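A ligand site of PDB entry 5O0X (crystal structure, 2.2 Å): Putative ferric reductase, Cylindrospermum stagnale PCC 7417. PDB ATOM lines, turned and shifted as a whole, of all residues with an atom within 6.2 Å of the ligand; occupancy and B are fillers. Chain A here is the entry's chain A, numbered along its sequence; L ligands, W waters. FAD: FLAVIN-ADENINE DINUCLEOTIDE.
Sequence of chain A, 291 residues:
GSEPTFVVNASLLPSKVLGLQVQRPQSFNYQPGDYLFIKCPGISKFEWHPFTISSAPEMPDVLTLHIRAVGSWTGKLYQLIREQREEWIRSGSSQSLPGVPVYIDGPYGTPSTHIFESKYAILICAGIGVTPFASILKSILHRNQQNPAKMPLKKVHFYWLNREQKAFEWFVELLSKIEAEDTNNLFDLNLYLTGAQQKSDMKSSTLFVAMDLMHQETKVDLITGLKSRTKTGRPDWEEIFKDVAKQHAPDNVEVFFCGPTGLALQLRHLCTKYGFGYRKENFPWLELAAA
The backbone carbonyl oxygen (O) of Arg 68 sits at hydrogen-bond distance from the side-chain hydroxyl (OG1) of Thr 74 (3.4 Å).
OG1 of Thr 74 sits at hydrogen-bond distance from N of Gly 71.
The side-chain hydroxyl (OG1) of Thr 74 lies within hydrogen-bond range of the backbone NH (N) of Val 70 (3.0 Å).
OG1 of Thr 131 is in hydrogen-bond range of O of Ile 128 (3.2 Å).
A ring nitrogen (NE2) of His 49 lies within hydrogen-bond range of the side-chain carboxylate (OE1) of Glu 47 (2.8 Å).
CD2 of Tyr 35 touches C7M of the ligand, 3.7 Å away.
Phe 51 touches the ligand (CA to N5, 3.5 Å).
CA of Ile 67 touches O2 of the ligand, 3.7 Å away.
Val 70 touches the ligand.
Gly 71 touches the ligand.
CG1 of Ile 128 touches N3 of the ligand (3.4 Å).
Trp 285 touches the ligand.
Of the 24 residues printed, 16 come within 4 Å of the ligand.
The nearest printed residue that does not touch the ligand is Gly 75 (4.5 Å).
Water W2 bridges O2 of the ligand (2.7 Å) and O of Arg 68 (2.8 Å).
Water W1 lies within hydrogen-bond range of the backbone carbonyl oxygen of Thr 52 (2.6 Å), an oxygen (O4) of the ligand (2.8 Å) and the backbone NH of His 66 (2.8 Å).
O of Pro 50 sits at hydrogen-bond distance from O2' of the ligand (2.5 Å).
N of Thr 74 sits at hydrogen-bond distance from O2P of the ligand, at 3.0 Å.
OG1 of Thr 74 is in hydrogen-bond range of O2P of the ligand (2.7 Å).
OG1 of Thr 131 is in hydrogen-bond range of O4 of the ligand (2.9 Å).
N3 of the ligand sits at hydrogen-bond distance from O of His 66, 3.0 Å away.
ND1 of His 49 is in hydrogen-bond range of O3' of the ligand, 3.0 Å away.
N of Arg 68 sits at hydrogen-bond distance from O2 of the ligand (3.0 Å).
The backbone NH of Trp 73 lies within hydrogen-bond range of an oxygen (O1P) of the ligand (3.1 Å).
The backbone NH (N) of Thr 52 lies within hydrogen-bond range of a nitrogen (N5) of the ligand, 3.2 Å away.
An oxygen (O2A) of the ligand is in hydrogen-bond range of the backbone NH (N) of Ser 72, 3.3 Å away.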
ATOM      1  N   TYR A  35      -0.715   8.438  -2.052  1.00  0.00           N
ATOM      2  CA  TYR A  35      -1.778   7.720  -1.365  1.00  0.00           C
ATOM      3  C   TYR A  35      -3.067   8.522  -1.344  1.00  0.00           C
ATOM      4  O   TYR A  35      -3.123   9.701  -1.767  1.00  0.00           O
ATOM      5  CB  TYR A  35      -1.333   7.338   0.030  1.00  0.00           C
ATOM      6  CG  TYR A  35      -1.070   8.478   1.004  1.00  0.00           C
ATOM      7  CD1 TYR A  35       0.136   9.182   0.974  1.00  0.00           C
ATOM      8  CD2 TYR A  35      -2.000   8.800   1.996  1.00  0.00           C
ATOM      9  CE1 TYR A  35       0.401  10.188   1.888  1.00  0.00           C
ATOM     10  CE2 TYR A  35      -1.763   9.804   2.929  1.00  0.00           C
ATOM     11  CZ  TYR A  35      -0.553  10.486   2.858  1.00  0.00           C
ATOM     12  OH  TYR A  35      -0.300  11.466   3.732  1.00  0.00           O
ATOM     13  N   PHE A  37      -7.089   8.792   1.100  1.00  0.00           N
ATOM     14  CA  PHE A  37      -7.940   8.361   2.212  1.00  0.00           C
ATOM     15  C   PHE A  37      -9.262   7.898   1.578  1.00  0.00           C
ATOM     16  O   PHE A  37      -9.766   8.514   0.615  1.00  0.00           O
ATOM     17  CB  PHE A  37      -8.226   9.479   3.209  1.00  0.00           C
ATOM     18  CG  PHE A  37      -7.092   9.764   4.154  1.00  0.00           C
ATOM     19  CD1 PHE A  37      -6.037  10.595   3.789  1.00  0.00           C
ATOM     20  CD2 PHE A  37      -7.075   9.182   5.390  1.00  0.00           C
ATOM     21  CE1 PHE A  37      -4.961  10.837   4.692  1.00  0.00           C
ATOM     22  CE2 PHE A  37      -6.024   9.406   6.286  1.00  0.00           C
ATOM     23  CZ  PHE A  37      -4.973  10.229   5.942  1.00  0.00           C
ATOM     24  N   GLU A  47     -15.341   7.189   9.341  1.00  0.00           N
ATOM     25  CA  GLU A  47     -13.904   6.950   9.332  1.00  0.00           C
ATOM     26  C   GLU A  47     -13.329   7.015   7.941  1.00  0.00           C
ATOM     27  O   GLU A  47     -13.920   6.524   6.974  1.00  0.00           O
ATOM     28  CB  GLU A  47     -13.538   5.612   9.940  1.00  0.00           C
ATOM     29  CG  GLU A  47     -13.716   5.509  11.417  1.00  0.00           C
ATOM     30  CD  GLU A  47     -13.048   4.272  12.008  1.00  0.00           C
ATOM     31  OE1 GLU A  47     -12.639   3.363  11.243  1.00  0.00           O
ATOM     32  OE2 GLU A  47     -12.900   4.206  13.266  1.00  0.00           O
ATOM     33  N   HIS A  49      -9.649   6.033   6.041  1.00  0.00           N
ATOM     34  CA  HIS A  49      -8.405   5.275   6.162  1.00  0.00           C
ATOM     35  C   HIS A  49      -7.496   5.485   4.965  1.00  0.00           C
ATOM     36  O   HIS A  49      -7.949   5.488   3.815  1.00  0.00           O
ATOM     37  CB  HIS A  49      -8.654   3.792   6.334  1.00  0.00           C
ATOM     38  CG  HIS A  49      -9.263   3.440   7.643  1.00  0.00           C
ATOM     39  ND1 HIS A  49      -8.548   2.841   8.652  1.00  0.00           N
ATOM     40  CD2 HIS A  49     -10.523   3.633   8.137  1.00  0.00           C
ATOM     41  CE1 HIS A  49      -9.335   2.655   9.697  1.00  0.00           C
ATOM     42  NE2 HIS A  49     -10.532   3.132   9.413  1.00  0.00           N
ATOM     43  N   PRO A  50      -6.196   5.679   5.225  1.00  0.00           N
ATOM     44  CA  PRO A  50      -5.203   5.895   4.186  1.00  0.00           C
ATOM     45  C   PRO A  50      -4.661   4.592   3.557  1.00  0.00           C
ATOM     46  O   PRO A  50      -4.340   3.651   4.259  1.00  0.00           O
ATOM     47  CB  PRO A  50      -4.084   6.630   4.916  1.00  0.00           C
ATOM     48  CG  PRO A  50      -4.159   6.133   6.311  1.00  0.00           C
ATOM     49  CD  PRO A  50      -5.596   5.845   6.572  1.00  0.00           C
ATOM     50  N   PHE A  51      -4.552   4.578   2.227  1.00  0.00           N
ATOM     51  CA  PHE A  51      -3.857   3.514   1.517  1.00  0.00           C
ATOM     52  C   PHE A  51      -3.119   4.074   0.324  1.00  0.00           C
ATOM     53  O   PHE A  51      -3.617   4.964  -0.382  1.00  0.00           O
ATOM     54  CB  PHE A  51      -4.825   2.404   1.045  1.00  0.00           C
ATOM     55  CG  PHE A  51      -5.654   1.799   2.142  1.00  0.00           C
ATOM     56  CD1 PHE A  51      -5.114   0.828   2.942  1.00  0.00           C
ATOM     57  CD2 PHE A  51      -6.950   2.275   2.434  1.00  0.00           C
ATOM     58  CE1 PHE A  51      -5.847   0.262   3.979  1.00  0.00           C
ATOM     59  CE2 PHE A  51      -7.680   1.722   3.466  1.00  0.00           C
ATOM     60  CZ  PHE A  51      -7.132   0.717   4.241  1.00  0.00           C
ATOM     61  N   THR A  52      -1.950   3.505   0.060  1.00  0.00           N
ATOM     62  CA  THR A  52      -1.164   3.857  -1.118  1.00  0.00           C
ATOM     63  C   THR A  52      -1.926   3.390  -2.350  1.00  0.00           C
ATOM     64  O   THR A  52      -2.505   2.322  -2.325  1.00  0.00           O
ATOM     65  CB  THR A  52       0.239   3.201  -1.064  1.00  0.00           C
ATOM     66  OG1 THR A  52       0.986   3.698   0.055  1.00  0.00           O
ATOM     67  CG2 THR A  52       0.999   3.446  -2.287  1.00  0.00           C
ATOM     68  N   ILE A  53      -1.888   4.172  -3.419  1.00  0.00           N
ATOM     69  CA  ILE A  53      -2.416   3.797  -4.733  1.00  0.00           C
ATOM     70  C   ILE A  53      -1.417   2.858  -5.431  1.00  0.00           C
ATOM     71  O   ILE A  53      -0.317   3.270  -5.767  1.00  0.00           O
ATOM     72  CB  ILE A  53      -2.705   5.025  -5.589  1.00  0.00           C
ATOM     73  CG1 ILE A  53      -3.745   5.918  -4.901  1.00  0.00           C
ATOM     74  CG2 ILE A  53      -3.259   4.627  -6.925  1.00  0.00           C
ATOM     75  CD1 ILE A  53      -3.777   7.350  -5.401  1.00  0.00           C
ATOM     76  N   HIS A  66      -4.290  -2.049  -2.459  1.00  0.00           N
ATOM     77  CA  HIS A  66      -4.089  -3.351  -1.883  1.00  0.00           C
ATOM     78  C   HIS A  66      -4.144  -3.186  -0.371  1.00  0.00           C
ATOM     79  O   HIS A  66      -3.199  -2.688   0.234  1.00  0.00           O
ATOM     80  CB  HIS A  66      -2.740  -3.952  -2.304  1.00  0.00           C
ATOM     81  CG  HIS A  66      -2.736  -4.505  -3.678  1.00  0.00           C
ATOM     82  ND1 HIS A  66      -2.850  -3.713  -4.802  1.00  0.00           N
ATOM     83  CD2 HIS A  66      -2.663  -5.785  -4.121  1.00  0.00           C
ATOM     84  CE1 HIS A  66      -2.858  -4.480  -5.875  1.00  0.00           C
ATOM     85  NE2 HIS A  66      -2.741  -5.738  -5.498  1.00  0.00           N
ATOM     86  N   ILE A  67      -5.246  -3.665   0.206  1.00  0.00           N
ATOM     87  CA  ILE A  67      -5.609  -3.468   1.619  1.00  0.00           C
ATOM     88  C   ILE A  67      -5.526  -4.741   2.395  1.00  0.00           C
ATOM     89  O   ILE A  67      -6.293  -5.658   2.173  1.00  0.00           O
ATOM     90  CB  ILE A  67      -7.060  -2.931   1.706  1.00  0.00           C
ATOM     91  CG1 ILE A  67      -7.143  -1.582   0.996  1.00  0.00           C
ATOM     92  CG2 ILE A  67      -7.513  -2.854   3.168  1.00  0.00           C
ATOM     93  CD1 ILE A  67      -8.527  -1.037   0.808  1.00  0.00           C
ATOM     94  N   ARG A  68      -4.633  -4.793   3.374  1.00  0.00           N
ATOM     95  CA  ARG A  68      -4.484  -5.967   4.204  1.00  0.00           C
ATOM     96  C   ARG A  68      -5.343  -5.880   5.438  1.00  0.00           C
ATOM     97  O   ARG A  68      -5.268  -4.888   6.214  1.00  0.00           O
ATOM     98  CB  ARG A  68      -3.025  -6.083   4.641  1.00  0.00           C
ATOM     99  CG  ARG A  68      -2.670  -7.390   5.312  1.00  0.00           C
ATOM    100  CD  ARG A  68      -1.222  -7.768   5.050  1.00  0.00           C
ATOM    101  NE  ARG A  68      -0.962  -9.062   5.654  1.00  0.00           N
ATOM    102  CZ  ARG A  68      -0.641  -9.257   6.926  1.00  0.00           C
ATOM    103  NH1 ARG A  68      -0.419  -8.249   7.766  1.00  0.00           N
ATOM    104  NH2 ARG A  68      -0.503 -10.494   7.363  1.00  0.00           N
ATOM    105  N   ALA A  69      -6.140  -6.931   5.655  1.00  0.00           N
ATOM    106  CA  ALA A  69      -7.030  -7.029   6.815  1.00  0.00           C
ATOM    107  C   ALA A  69      -6.263  -7.306   8.078  1.00  0.00           C
ATOM    108  O   ALA A  69      -5.918  -8.425   8.346  1.00  0.00           O
ATOM    109  CB  ALA A  69      -8.043  -8.123   6.592  1.00  0.00           C
ATOM    110  N   VAL A  70      -5.988  -6.269   8.837  1.00  0.00           N
ATOM    111  CA  VAL A  70      -5.209  -6.382  10.052  1.00  0.00           C
ATOM    112  C   VAL A  70      -5.974  -5.948  11.296  1.00  0.00           C
ATOM    113  O   VAL A  70      -5.461  -5.965  12.409  1.00  0.00           O
ATOM    114  CB  VAL A  70      -3.933  -5.503   9.978  1.00  0.00           C
ATOM    115  CG1 VAL A  70      -3.020  -5.992   8.858  1.00  0.00           C
ATOM    116  CG2 VAL A  70      -4.298  -4.024   9.810  1.00  0.00           C
ATOM    117  N   GLY A  71      -7.180  -5.465  11.119  1.00  0.00           N
ATOM    118  CA  GLY A  71      -7.911  -4.942  12.243  1.00  0.00           C
ATOM    119  C   GLY A  71      -9.343  -4.684  11.862  1.00  0.00           C
ATOM    120  O   GLY A  71      -9.864  -5.252  10.886  1.00  0.00           O
ATOM    121  N   SER A  72      -9.931  -3.747  12.580  1.00  0.00           N
ATOM    122  CA  SER A  72     -11.362  -3.560  12.600  1.00  0.00           C
ATOM    123  C   SER A  72     -11.965  -3.113  11.265  1.00  0.00           C
ATOM    124  O   SER A  72     -12.902  -3.737  10.732  1.00  0.00           O
ATOM    125  CB  SER A  72     -11.705  -2.580  13.738  1.00  0.00           C
ATOM    126  OG  SER A  72     -13.009  -2.111  13.576  1.00  0.00           O
ATOM    127  N   TRP A  73     -11.487  -1.990  10.729  1.00  0.00           N
ATOM    128  CA  TRP A  73     -12.125  -1.461   9.525  1.00  0.00           C
ATOM    129  C   TRP A  73     -11.747  -2.321   8.288  1.00  0.00           C
ATOM    130  O   TRP A  73     -12.604  -2.653   7.465  1.00  0.00           O
ATOM    131  CB  TRP A  73     -11.736  -0.008   9.359  1.00  0.00           C
ATOM    132  CG  TRP A  73     -12.371   0.729   8.227  1.00  0.00           C
ATOM    133  CD1 TRP A  73     -13.429   1.582   8.302  1.00  0.00           C
ATOM    134  CD2 TRP A  73     -11.950   0.742   6.850  1.00  0.00           C
ATOM    135  NE1 TRP A  73     -13.703   2.116   7.072  1.00  0.00           N
ATOM    136  CE2 TRP A  73     -12.816   1.609   6.158  1.00  0.00           C
ATOM    137  CE3 TRP A  73     -10.928   0.113   6.154  1.00  0.00           C
ATOM    138  CZ2 TRP A  73     -12.702   1.853   4.798  1.00  0.00           C
ATOM    139  CZ3 TRP A  73     -10.826   0.338   4.770  1.00  0.00           C
ATOM    140  CH2 TRP A  73     -11.690   1.210   4.119  1.00  0.00           C
ATOM    141  N   THR A  74     -10.471  -2.646   8.158  1.00  0.00           N
ATOM    142  CA  THR A  74      -9.977  -3.444   7.024  1.00  0.00           C
ATOM    143  C   THR A  74     -10.556  -4.870   7.081  1.00  0.00           C
ATOM    144  O   THR A  74     -10.970  -5.386   6.052  1.00  0.00           O
ATOM    145  CB  THR A  74      -8.420  -3.503   6.988  1.00  0.00           C
ATOM    146  OG1 THR A  74      -7.897  -4.003   8.229  1.00  0.00           O
ATOM    147  CG2 THR A  74      -7.842  -2.130   6.718  1.00  0.00           C
ATOM    148  N   GLY A  75     -10.629  -5.462   8.258  1.00  0.00           N
ATOM    149  CA  GLY A  75     -11.296  -6.742   8.429  1.00  0.00           C
ATOM    150  C   GLY A  75     -12.762  -6.735   8.004  1.00  0.00           C
ATOM    151  O   GLY A  75     -13.211  -7.651   7.300  1.00  0.00           O
ATOM    152  N   THR A 110       4.231  11.856  -1.369  1.00  0.00           N
ATOM    153  CA  THR A 110       5.334  11.280  -0.592  1.00  0.00           C
ATOM    154  C   THR A 110       6.660  11.540  -1.295  1.00  0.00           C
ATOM    155  O   THR A 110       6.731  11.787  -2.517  1.00  0.00           O
ATOM    156  CB  THR A 110       5.239   9.757  -0.363  1.00  0.00           C
ATOM    157  OG1 THR A 110       5.547   9.039  -1.557  1.00  0.00           O
ATOM    158  CG2 THR A 110       3.837   9.359   0.110  1.00  0.00           C
ATOM    159  N   ILE A 128       3.236  -5.412   3.066  1.00  0.00           N
ATOM    160  CA  ILE A 128       2.337  -4.546   2.295  1.00  0.00           C
ATOM    161  C   ILE A 128       2.993  -3.189   2.043  1.00  0.00           C
ATOM    162  O   ILE A 128       2.507  -2.406   1.232  1.00  0.00           O
ATOM    163  CB  ILE A 128       0.943  -4.406   2.987  1.00  0.00           C
ATOM    164  CG1 ILE A 128      -0.121  -3.951   2.013  1.00  0.00           C
ATOM    165  CG2 ILE A 128       0.958  -3.510   4.225  1.00  0.00           C
ATOM    166  CD1 ILE A 128      -0.303  -4.940   0.864  1.00  0.00           C
ATOM    167  N   THR A 131       3.538  -1.479  -1.668  1.00  0.00           N
ATOM    168  CA  THR A 131       2.574  -0.852  -2.569  1.00  0.00           C
ATOM    169  C   THR A 131       3.030   0.426  -3.265  1.00  0.00           C
ATOM    170  O   THR A 131       2.744   0.592  -4.454  1.00  0.00           O
ATOM    171  CB  THR A 131       1.218  -0.650  -1.842  1.00  0.00           C
ATOM    172  OG1 THR A 131       1.404  -0.039  -0.574  1.00  0.00           O
ATOM    173  CG2 THR A 131       0.526  -1.980  -1.587  1.00  0.00           C
ATOM    174  N   PRO A 132       3.716   1.361  -2.559  1.00  0.00           N
ATOM    175  CA  PRO A 132       4.159   2.524  -3.334  1.00  0.00           C
ATOM    176  C   PRO A 132       5.147   2.144  -4.433  1.00  0.00           C
ATOM    177  O   PRO A 132       5.171   2.761  -5.479  1.00  0.00           O
ATOM    178  CB  PRO A 132       4.860   3.429  -2.301  1.00  0.00           C
ATOM    179  CG  PRO A 132       5.097   2.552  -1.093  1.00  0.00           C
ATOM    180  CD  PRO A 132       4.023   1.491  -1.126  1.00  0.00           C
ATOM    181  N   PRO A 284       4.007   3.076  10.913  1.00  0.00           N
ATOM    182  CA  PRO A 284       3.502   2.343  12.087  1.00  0.00           C
ATOM    183  C   PRO A 284       2.679   1.086  11.787  1.00  0.00           C
ATOM    184  O   PRO A 284       2.624   0.183  12.586  1.00  0.00           O
ATOM    185  CB  PRO A 284       2.619   3.406  12.819  1.00  0.00           C
ATOM    186  CG  PRO A 284       3.135   4.740  12.348  1.00  0.00           C
ATOM    187  CD  PRO A 284       3.568   4.490  10.905  1.00  0.00           C
ATOM    188  N   TRP A 285       2.016   1.053  10.652  1.00  0.00           N
ATOM    189  CA  TRP A 285       1.315  -0.140  10.229  1.00  0.00           C
ATOM    190  C   TRP A 285       2.225  -1.283   9.797  1.00  0.00           C
ATOM    191  O   TRP A 285       1.727  -2.363   9.566  1.00  0.00           O
ATOM    192  CB  TRP A 285       0.308   0.202   9.124  1.00  0.00           C
ATOM    193  CG  TRP A 285       0.922   0.586   7.798  1.00  0.00           C
ATOM    194  CD1 TRP A 285       1.073  -0.230   6.713  1.00  0.00           C
ATOM    195  CD2 TRP A 285       1.407   1.861   7.407  1.00  0.00           C
ATOM    196  NE1 TRP A 285       1.584   0.458   5.669  1.00  0.00           N
ATOM    197  CE2 TRP A 285       1.842   1.746   6.072  1.00  0.00           C
ATOM    198  CE3 TRP A 285       1.493   3.116   8.054  1.00  0.00           C
ATOM    199  CZ2 TRP A 285       2.352   2.811   5.360  1.00  0.00           C
ATOM    200  CZ3 TRP A 285       1.999   4.173   7.364  1.00  0.00           C
ATOM    201  CH2 TRP A 285       2.441   4.030   6.020  1.00  0.00           C
HETATM  202  PA  FAD L   1      -6.859  -1.161  13.433  1.00  0.00           P
HETATM  203  O1A FAD L   1      -6.496   0.197  13.595  1.00  0.00           O
HETATM  204  O2A FAD L   1      -7.943  -1.679  14.242  1.00  0.00           O
HETATM  205  O5B FAD L   1      -5.631  -1.990  13.796  1.00  0.00           O
HETATM  206  C5B FAD L   1      -4.392  -1.388  13.648  1.00  0.00           C
HETATM  207  C4B FAD L   1      -3.305  -2.220  14.284  1.00  0.00           C
HETATM  208  O4B FAD L   1      -3.125  -1.822  15.627  1.00  0.00           O
HETATM  209  C3B FAD L   1      -3.654  -3.659  14.337  1.00  0.00           C
HETATM  210  O3B FAD L   1      -2.434  -4.335  14.309  1.00  0.00           O
HETATM  211  C2B FAD L   1      -4.225  -3.800  15.711  1.00  0.00           C
HETATM  212  O2B FAD L   1      -4.075  -5.090  16.232  1.00  0.00           O
HETATM  213  C1B FAD L   1      -3.437  -2.841  16.509  1.00  0.00           C
HETATM  214  N9A FAD L   1      -4.421  -2.348  17.462  1.00  0.00           N
HETATM  215  C8A FAD L   1      -5.654  -1.993  17.151  1.00  0.00           C
HETATM  216  N7A FAD L   1      -6.358  -1.592  18.205  1.00  0.00           N
HETATM  217  C5A FAD L   1      -5.543  -1.695  19.242  1.00  0.00           C
HETATM  218  C6A FAD L   1      -5.664  -1.437  20.674  1.00  0.00           C
HETATM  219  N6A FAD L   1      -6.797  -0.987  21.221  1.00  0.00           N
HETATM  220  N1A FAD L   1      -4.586  -1.672  21.412  1.00  0.00           N
HETATM  221  C2A FAD L   1      -3.441  -2.131  20.894  1.00  0.00           C
HETATM  222  N3A FAD L   1      -3.266  -2.392  19.596  1.00  0.00           N
HETATM  223  C4A FAD L   1      -4.276  -2.196  18.751  1.00  0.00           C
HETATM  224  N1  FAD L   1      -2.306  -0.471   4.589  1.00  0.00           N
HETATM  225  C2  FAD L   1      -2.347  -1.364   3.623  1.00  0.00           C
HETATM  226  O2  FAD L   1      -2.796  -2.452   3.863  1.00  0.00           O
HETATM  227  N3  FAD L   1      -1.952  -1.123   2.402  1.00  0.00           N
HETATM  228  C4  FAD L   1      -1.465   0.014   2.062  1.00  0.00           C
HETATM  229  O4  FAD L   1      -1.110   0.176   0.920  1.00  0.00           O
HETATM  230  C4X FAD L   1      -1.368   1.074   3.095  1.00  0.00           C
HETATM  231  N5  FAD L   1      -0.868   2.267   2.816  1.00  0.00           N
HETATM  232  C5X FAD L   1      -0.816   3.193   3.753  1.00  0.00           C
HETATM  233  C6  FAD L   1      -0.318   4.405   3.412  1.00  0.00           C
HETATM  234  C7  FAD L   1      -0.215   5.411   4.330  1.00  0.00           C
HETATM  235  C7M FAD L   1       0.343   6.741   3.934  1.00  0.00           C
HETATM  236  C8  FAD L   1      -0.664   5.164   5.698  1.00  0.00           C
HETATM  237  C8M FAD L   1      -0.571   6.265   6.712  1.00  0.00           C
HETATM  238  C9  FAD L   1      -1.179   3.936   6.044  1.00  0.00           C
HETATM  239  C9A FAD L   1      -1.278   2.918   5.142  1.00  0.00           C
HETATM  240  N10 FAD L   1      -1.790   1.649   5.482  1.00  0.00           N
HETATM  241  C10 FAD L   1      -1.842   0.750   4.439  1.00  0.00           C
HETATM  242  C1' FAD L   1      -2.322   1.287   6.802  1.00  0.00           C
HETATM  243  C2' FAD L   1      -3.865   1.511   6.814  1.00  0.00           C
HETATM  244  O2' FAD L   1      -4.137   2.860   6.654  1.00  0.00           O
HETATM  245  C3' FAD L   1      -4.924   1.022   7.875  1.00  0.00           C
HETATM  246  O3' FAD L   1      -5.707   1.979   8.607  1.00  0.00           O
HETATM  247  C4' FAD L   1      -4.507   0.188   8.993  1.00  0.00           C
HETATM  248  O4' FAD L   1      -3.485  -0.557   8.390  1.00  0.00           O
HETATM  249  C5' FAD L   1      -5.731  -0.612   9.473  1.00  0.00           C
HETATM  250  O5' FAD L   1      -6.897  -0.017  10.081  1.00  0.00           O
HETATM  251  P   FAD L   1      -7.956  -0.927  10.842  1.00  0.00           P
HETATM  252  O1P FAD L   1      -9.031  -0.231  11.436  1.00  0.00           O
HETATM  253  O2P FAD L   1      -8.303  -2.054  10.076  1.00  0.00           O
HETATM  254  O3P FAD L   1      -7.103  -1.577  11.955  1.00  0.00           O
HETATM  255  O   HOH W   1      -2.508  -0.126  -1.475  1.00  0.00           O
HETATM  256  O   HOH W   2      -3.911  -2.422   6.364  1.00  0.00           O
HETATM  257  O   HOH W   3      -2.481  -1.010  10.723  1.00  0.00           O
HETATM  258  O   HOH W   4      -2.257   3.510   9.502  1.00  0.00           O
